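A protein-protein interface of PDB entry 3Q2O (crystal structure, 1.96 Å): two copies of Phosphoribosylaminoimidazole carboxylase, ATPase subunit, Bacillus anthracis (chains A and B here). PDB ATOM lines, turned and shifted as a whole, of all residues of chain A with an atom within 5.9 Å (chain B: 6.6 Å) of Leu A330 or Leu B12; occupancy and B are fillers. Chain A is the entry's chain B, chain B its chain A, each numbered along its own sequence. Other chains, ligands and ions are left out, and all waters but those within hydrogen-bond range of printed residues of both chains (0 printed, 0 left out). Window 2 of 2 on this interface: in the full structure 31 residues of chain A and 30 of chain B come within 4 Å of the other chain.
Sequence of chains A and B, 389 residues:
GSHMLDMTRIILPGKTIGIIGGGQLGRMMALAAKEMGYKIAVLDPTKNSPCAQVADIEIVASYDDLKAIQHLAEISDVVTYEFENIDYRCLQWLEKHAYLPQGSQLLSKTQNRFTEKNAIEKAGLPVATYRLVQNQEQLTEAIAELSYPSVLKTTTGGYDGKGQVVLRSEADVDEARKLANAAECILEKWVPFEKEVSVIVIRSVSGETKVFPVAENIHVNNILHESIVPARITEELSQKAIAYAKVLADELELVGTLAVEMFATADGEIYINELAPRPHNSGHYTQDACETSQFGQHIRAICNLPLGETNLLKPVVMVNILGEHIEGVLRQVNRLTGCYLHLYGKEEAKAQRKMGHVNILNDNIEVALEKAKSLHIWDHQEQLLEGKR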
ATOM      1  N   HIS A 325     -17.100  -4.644 -14.661  1.00  0.00           N
ATOM      2  CA  HIS A 325     -15.953  -3.795 -14.296  1.00  0.00           C
ATOM      3  C   HIS A 325     -15.914  -3.367 -12.827  1.00  0.00           C
ATOM      4  O   HIS A 325     -14.843  -3.005 -12.331  1.00  0.00           O
ATOM      5  CB  HIS A 325     -15.870  -2.532 -15.169  1.00  0.00           C
ATOM      6  CG  HIS A 325     -15.875  -2.803 -16.640  1.00  0.00           C
ATOM      7  ND1 HIS A 325     -16.897  -2.391 -17.464  1.00  0.00           N
ATOM      8  CD2 HIS A 325     -14.980  -3.436 -17.436  1.00  0.00           C
ATOM      9  CE1 HIS A 325     -16.641  -2.770 -18.705  1.00  0.00           C
ATOM     10  NE2 HIS A 325     -15.481  -3.402 -18.715  1.00  0.00           N
ATOM     11  N   ILE A 326     -17.073  -3.392 -12.158  1.00  0.00           N
ATOM     12  CA  ILE A 326     -17.234  -2.827 -10.802  1.00  0.00           C
ATOM     13  C   ILE A 326     -16.234  -3.380  -9.771  1.00  0.00           C
ATOM     14  O   ILE A 326     -15.663  -2.622  -8.992  1.00  0.00           O
ATOM     15  CB  ILE A 326     -18.729  -2.912 -10.288  1.00  0.00           C
ATOM     16  CG1 ILE A 326     -18.942  -2.103  -8.998  1.00  0.00           C
ATOM     17  CG2 ILE A 326     -19.176  -4.360 -10.062  1.00  0.00           C
ATOM     18  CD1 ILE A 326     -18.818  -0.600  -9.164  1.00  0.00           C
ATOM     19  N   GLU A 327     -16.019  -4.695  -9.779  1.00  0.00           N
ATOM     20  CA  GLU A 327     -15.023  -5.317  -8.905  1.00  0.00           C
ATOM     21  C   GLU A 327     -13.641  -4.700  -9.148  1.00  0.00           C
ATOM     22  O   GLU A 327     -12.960  -4.297  -8.205  1.00  0.00           O
ATOM     23  CB  GLU A 327     -15.000  -6.839  -9.112  1.00  0.00           C
ATOM     24  CG  GLU A 327     -13.991  -7.604  -8.252  1.00  0.00           C
ATOM     25  CD  GLU A 327     -14.066  -9.121  -8.465  1.00  0.00           C
ATOM     26  OE1 GLU A 327     -15.128  -9.626  -8.912  1.00  0.00           O
ATOM     27  OE2 GLU A 327     -13.058  -9.811  -8.182  1.00  0.00           O
ATOM     28  N   GLY A 328     -13.254  -4.604 -10.417  1.00  0.00           N
ATOM     29  CA  GLY A 328     -11.982  -4.005 -10.805  1.00  0.00           C
ATOM     30  C   GLY A 328     -11.846  -2.551 -10.376  1.00  0.00           C
ATOM     31  O   GLY A 328     -10.779  -2.134  -9.929  1.00  0.00           O
ATOM     32  N   VAL A 329     -12.923  -1.780 -10.524  1.00  0.00           N
ATOM     33  CA  VAL A 329     -12.939  -0.378 -10.084  1.00  0.00           C
ATOM     34  C   VAL A 329     -12.659  -0.283  -8.569  1.00  0.00           C
ATOM     35  O   VAL A 329     -11.757   0.445  -8.133  1.00  0.00           O
ATOM     36  CB  VAL A 329     -14.277   0.324 -10.473  1.00  0.00           C
ATOM     37  CG1 VAL A 329     -14.376   1.723  -9.826  1.00  0.00           C
ATOM     38  CG2 VAL A 329     -14.415   0.424 -12.000  1.00  0.00           C
ATOM     39  N   LEU A 330     -13.407  -1.057  -7.786  1.00  0.00           N
ATOM     40  CA  LEU A 330     -13.293  -1.023  -6.324  1.00  0.00           C
ATOM     41  C   LEU A 330     -11.930  -1.490  -5.821  1.00  0.00           C
ATOM     42  O   LEU A 330     -11.394  -0.918  -4.869  1.00  0.00           O
ATOM     43  CB  LEU A 330     -14.433  -1.815  -5.669  1.00  0.00           C
ATOM     44  CG  LEU A 330     -15.852  -1.282  -5.913  1.00  0.00           C
ATOM     45  CD1 LEU A 330     -16.907  -2.281  -5.430  1.00  0.00           C
ATOM     46  CD2 LEU A 330     -16.069   0.092  -5.272  1.00  0.00           C
ATOM     47  N   ARG A 331     -11.364  -2.504  -6.479  1.00  0.00           N
ATOM     48  CA  ARG A 331     -10.018  -2.997  -6.166  1.00  0.00           C
ATOM     49  C   ARG A 331      -8.934  -1.993  -6.549  1.00  0.00           C
ATOM     50  O   ARG A 331      -7.863  -1.962  -5.940  1.00  0.00           O
ATOM     51  CB  ARG A 331      -9.752  -4.327  -6.888  1.00  0.00           C
ATOM     52  CG  ARG A 331     -10.088  -5.589  -6.086  1.00  0.00           C
ATOM     53  CD  ARG A 331      -9.998  -6.889  -6.952  1.00  0.00           C
ATOM     54  NE  ARG A 331      -9.122  -6.749  -8.122  1.00  0.00           N
ATOM     55  CZ  ARG A 331      -9.477  -7.009  -9.380  1.00  0.00           C
ATOM     56  NH1 ARG A 331     -10.695  -7.463  -9.665  1.00  0.00           N
ATOM     57  NH2 ARG A 331      -8.603  -6.829 -10.363  1.00  0.00           N
ATOM     58  N   GLN A 332      -9.215  -1.184  -7.567  1.00  0.00           N
ATOM     59  CA  GLN A 332      -8.248  -0.223  -8.092  1.00  0.00           C
ATOM     60  C   GLN A 332      -8.548   1.235  -7.704  1.00  0.00           C
ATOM     61  O   GLN A 332      -8.027   2.158  -8.344  1.00  0.00           O
ATOM     62  CB  GLN A 332      -8.159  -0.331  -9.624  1.00  0.00           C
ATOM     63  CG  GLN A 332      -7.516  -1.606 -10.179  1.00  0.00           C
ATOM     64  CD  GLN A 332      -6.015  -1.473 -10.308  1.00  0.00           C
ATOM     65  OE1 GLN A 332      -5.503  -1.124 -11.376  1.00  0.00           O
ATOM     66  NE2 GLN A 332      -5.300  -1.715  -9.211  1.00  0.00           N
ATOM     67  N   VAL A 333      -9.364   1.452  -6.668  1.00  0.00           N
ATOM     68  CA  VAL A 333      -9.755   2.827  -6.284  1.00  0.00           C
ATOM     69  C   VAL A 333      -8.564   3.729  -5.978  1.00  0.00           C
ATOM     70  O   VAL A 333      -8.624   4.920  -6.235  1.00  0.00           O
ATOM     71  CB  VAL A 333     -10.756   2.924  -5.094  1.00  0.00           C
ATOM     72  CG1 VAL A 333     -12.131   2.382  -5.467  1.00  0.00           C
ATOM     73  CG2 VAL A 333     -10.189   2.275  -3.820  1.00  0.00           C
ATOM     74  N   ASN A 334      -7.502   3.142  -5.431  1.00  0.00           N
ATOM     75  CA  ASN A 334      -6.269   3.843  -5.070  1.00  0.00           C
ATOM     76  C   ASN A 334      -5.512   4.419  -6.277  1.00  0.00           C
ATOM     77  O   ASN A 334      -4.653   5.295  -6.133  1.00  0.00           O
ATOM     78  CB  ASN A 334      -5.354   2.891  -4.283  1.00  0.00           C
ATOM     79  CG  ASN A 334      -5.175   1.543  -4.979  1.00  0.00           C
ATOM     80  OD1 ASN A 334      -6.151   0.860  -5.314  1.00  0.00           O
ATOM     81  ND2 ASN A 334      -3.924   1.154  -5.200  1.00  0.00           N
ATOM     82  N   LEU A 343     -20.924   6.580  -9.410  1.00  0.00           N
ATOM     83  CA  LEU A 343     -21.543   5.274  -9.233  1.00  0.00           C
ATOM     84  C   LEU A 343     -23.005   5.424  -8.852  1.00  0.00           C
ATOM     85  O   LEU A 343     -23.355   6.243  -7.997  1.00  0.00           O
ATOM     86  CB  LEU A 343     -20.788   4.438  -8.194  1.00  0.00           C
ATOM     87  CG  LEU A 343     -19.379   3.994  -8.617  1.00  0.00           C
ATOM     88  CD1 LEU A 343     -18.615   3.485  -7.403  1.00  0.00           C
ATOM     89  CD2 LEU A 343     -19.446   2.925  -9.711  1.00  0.00           C
ATOM     90  N   ILE B  10      -9.459   2.346   3.769  1.00  0.00           N
ATOM     91  CA  ILE B  10     -10.282   2.950   2.715  1.00  0.00           C
ATOM     92  C   ILE B  10     -11.755   2.644   2.937  1.00  0.00           C
ATOM     93  O   ILE B  10     -12.127   1.495   3.234  1.00  0.00           O
ATOM     94  CB  ILE B  10      -9.865   2.465   1.294  1.00  0.00           C
ATOM     95  CG1 ILE B  10      -8.414   2.861   0.980  1.00  0.00           C
ATOM     96  CG2 ILE B  10     -10.826   2.987   0.216  1.00  0.00           C
ATOM     97  CD1 ILE B  10      -7.798   2.137  -0.268  1.00  0.00           C
ATOM     98  N   ILE B  11     -12.587   3.675   2.798  1.00  0.00           N
ATOM     99  CA  ILE B  11     -14.041   3.536   2.876  1.00  0.00           C
ATOM    100  C   ILE B  11     -14.596   3.580   1.447  1.00  0.00           C
ATOM    101  O   ILE B  11     -14.614   4.631   0.810  1.00  0.00           O
ATOM    102  CB  ILE B  11     -14.697   4.646   3.755  1.00  0.00           C
ATOM    103  CG1 ILE B  11     -13.988   4.791   5.115  1.00  0.00           C
ATOM    104  CG2 ILE B  11     -16.211   4.413   3.904  1.00  0.00           C
ATOM    105  CD1 ILE B  11     -14.084   3.549   6.067  1.00  0.00           C
ATOM    106  N   LEU B  12     -15.021   2.422   0.954  1.00  0.00           N
ATOM    107  CA  LEU B  12     -15.439   2.265  -0.444  1.00  0.00           C
ATOM    108  C   LEU B  12     -16.833   2.775  -0.708  1.00  0.00           C
ATOM    109  O   LEU B  12     -17.674   2.754   0.187  1.00  0.00           O
ATOM    110  CB  LEU B  12     -15.375   0.787  -0.854  1.00  0.00           C
ATOM    111  CG  LEU B  12     -13.963   0.198  -0.889  1.00  0.00           C
ATOM    112  CD1 LEU B  12     -14.004  -1.330  -1.069  1.00  0.00           C
ATOM    113  CD2 LEU B  12     -13.146   0.872  -1.991  1.00  0.00           C
ATOM    114  N   PRO B  13     -17.092   3.224  -1.951  1.00  0.00           N
ATOM    115  CA  PRO B  13     -18.450   3.484  -2.407  1.00  0.00           C
ATOM    116  C   PRO B  13     -19.380   2.351  -2.008  1.00  0.00           C
ATOM    117  O   PRO B  13     -18.988   1.180  -2.076  1.00  0.00           O
ATOM    118  CB  PRO B  13     -18.293   3.507  -3.925  1.00  0.00           C
ATOM    119  CG  PRO B  13     -16.936   4.149  -4.110  1.00  0.00           C
ATOM    120  CD  PRO B  13     -16.093   3.585  -2.977  1.00  0.00           C
ATOM    121  N   GLY B  14     -20.598   2.701  -1.604  1.00  0.00           N
ATOM    122  CA  GLY B  14     -21.562   1.715  -1.118  1.00  0.00           C
ATOM    123  C   GLY B  14     -21.657   1.735   0.393  1.00  0.00           C
ATOM    124  O   GLY B  14     -22.656   1.292   0.964  1.00  0.00           O
ATOM    125  N   LYS B  15     -20.611   2.231   1.051  1.00  0.00           N
ATOM    126  CA  LYS B  15     -20.634   2.392   2.512  1.00  0.00           C
ATOM    127  C   LYS B  15     -21.410   3.636   2.909  1.00  0.00           C
ATOM    128  O   LYS B  15     -21.740   4.460   2.062  1.00  0.00           O
ATOM    129  CB  LYS B  15     -19.217   2.454   3.087  1.00  0.00           C
ATOM    130  CG  LYS B  15     -18.389   1.181   2.883  1.00  0.00           C
ATOM    131  CD  LYS B  15     -19.030  -0.021   3.554  1.00  0.00           C
ATOM    132  CE  LYS B  15     -17.985  -1.115   3.809  1.00  0.00           C
ATOM    133  NZ  LYS B  15     -17.335  -1.528   2.535  1.00  0.00           N
ATOM    134  N   THR B  16     -21.683   3.769   4.204  1.00  0.00           N
ATOM    135  CA  THR B  16     -22.449   4.889   4.733  1.00  0.00           C
ATOM    136  C   THR B  16     -21.539   5.928   5.406  1.00  0.00           C
ATOM    137  O   THR B  16     -20.775   5.602   6.326  1.00  0.00           O
ATOM    138  CB  THR B  16     -23.485   4.403   5.775  1.00  0.00           C
ATOM    139  OG1 THR B  16     -24.390   3.482   5.157  1.00  0.00           O
ATOM    140  CG2 THR B  16     -24.276   5.587   6.363  1.00  0.00           C
ATOM    141  N   MET B  36     -20.786   9.571  -5.916  1.00  0.00           N
ATOM    142  CA  MET B  36     -19.793   8.523  -5.861  1.00  0.00           C
ATOM    143  C   MET B  36     -20.341   7.216  -5.304  1.00  0.00           C
ATOM    144  O   MET B  36     -19.587   6.282  -5.091  1.00  0.00           O
ATOM    145  CB  MET B  36     -18.572   8.975  -5.052  1.00  0.00           C
ATOM    146  CG  MET B  36     -17.596   9.843  -5.841  1.00  0.00           C
ATOM    147  SD  MET B  36     -16.151  10.293  -4.841  1.00  0.00           S
ATOM    148  CE  MET B  36     -16.857  11.524  -3.761  1.00  0.00           C
ATOM    149  N   GLY B  37     -21.644   7.175  -5.040  1.00  0.00           N
ATOM    150  CA  GLY B  37     -22.298   5.940  -4.654  1.00  0.00           C
ATOM    151  C   GLY B  37     -22.272   5.639  -3.165  1.00  0.00           C
ATOM    152  O   GLY B  37     -22.408   4.487  -2.787  1.00  0.00           O
ATOM    153  N   TYR B  38     -22.101   6.664  -2.324  1.00  0.00           N
ATOM    154  CA  TYR B  38     -22.190   6.478  -0.876  1.00  0.00           C
ATOM    155  C   TYR B  38     -23.608   6.652  -0.371  1.00  0.00           C
ATOM    156  O   TYR B  38     -24.409   7.386  -0.951  1.00  0.00           O
ATOM    157  CB  TYR B  38     -21.268   7.454  -0.117  1.00  0.00           C
ATOM    158  CG  TYR B  38     -19.809   7.146  -0.317  1.00  0.00           C
ATOM    159  CD1 TYR B  38     -19.150   6.222   0.499  1.00  0.00           C
ATOM    160  CD2 TYR B  38     -19.085   7.762  -1.341  1.00  0.00           C
ATOM    161  CE1 TYR B  38     -17.813   5.926   0.311  1.00  0.00           C
ATOM    162  CE2 TYR B  38     -17.734   7.465  -1.543  1.00  0.00           C
ATOM    163  CZ  TYR B  38     -17.110   6.553  -0.713  1.00  0.00           C
ATOM    164  OH  TYR B  38     -15.786   6.276  -0.904  1.00  0.00           O
ATOM    165  N   CYS B 303     -12.461   9.323   3.254  1.00  0.00           N
ATOM    166  CA  CYS B 303     -12.628   7.951   2.781  1.00  0.00           C
ATOM    167  C   CYS B 303     -11.300   7.364   2.299  1.00  0.00           C
ATOM    168  O   CYS B 303     -11.220   6.179   1.962  1.00  0.00           O
ATOM    169  CB  CYS B 303     -13.671   7.879   1.656  1.00  0.00           C
ATOM    170  SG  CYS B 303     -15.359   8.191   2.218  1.00  0.00           S
ATOM    171  N   LEU B 305      -9.653   8.110  -0.472  1.00  0.00           N
ATOM    172  CA  LEU B 305      -9.552   7.956  -1.923  1.00  0.00           C
ATOM    173  C   LEU B 305      -8.493   8.927  -2.435  1.00  0.00           C
ATOM    174  O   LEU B 305      -8.133   9.875  -1.721  1.00  0.00           O
ATOM    175  CB  LEU B 305     -10.896   8.256  -2.583  1.00  0.00           C
ATOM    176  CG  LEU B 305     -12.118   7.526  -2.028  1.00  0.00           C
ATOM    177  CD1 LEU B 305     -13.394   7.997  -2.720  1.00  0.00           C
ATOM    178  CD2 LEU B 305     -11.962   6.005  -2.181  1.00  0.00           C
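The backbone carbonyl oxygen (O) of Gly B37 lies within hydrogen-bond range of the backbone NH (N) of Gly B14, at 2.8 Å.
Leu B12 touches Leu A330.
CD2 of Leu B12 touches CG2 of Val A333 (3.7 Å).
CB of Pro B13 touches CD1 of Leu A343, at 3.5 Å.
Leu A343 touches Met B36 (CD1 to O, 3.8 Å).
Leu A343 touches Gly B37.
Of chain B, only Leu B12 (3.8 Å) comes within 4 Å of Leu A330.
Printed residues of chain B within 4 Å of Val A333: Leu B12.
Asn A334 touches none of the printed residues of chain B.
Of the printed residues of chain B, Leu A343 touches Pro B13 (3.5 Å), Met B36 (3.8 Å) and Gly B37 (3.5 Å).
Of the printed residues of chain A, Pro B13 touches Leu A343 (3.5 Å).
Of the printed residues of chain A, Met B36 touches Leu A343.
The nearest residue of chain B that does not touch Leu A330 is Pro B13 (4.2 Å).
The nearest printed residue of chain A that does not touch Leu B12 is Arg A331 (5.9 Å).
Hydrophobic or aromatic side chains of chain B that line the printed part of chain A: Leu B12 and Pro B13.
Hydrophobic or aromatic side chains of chain A within 4 Å of the printed part of chain B: Val A333 and Leu A343.
Among the printed residues, 5 pairs touch across the chains.
No position is printed for both chains.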
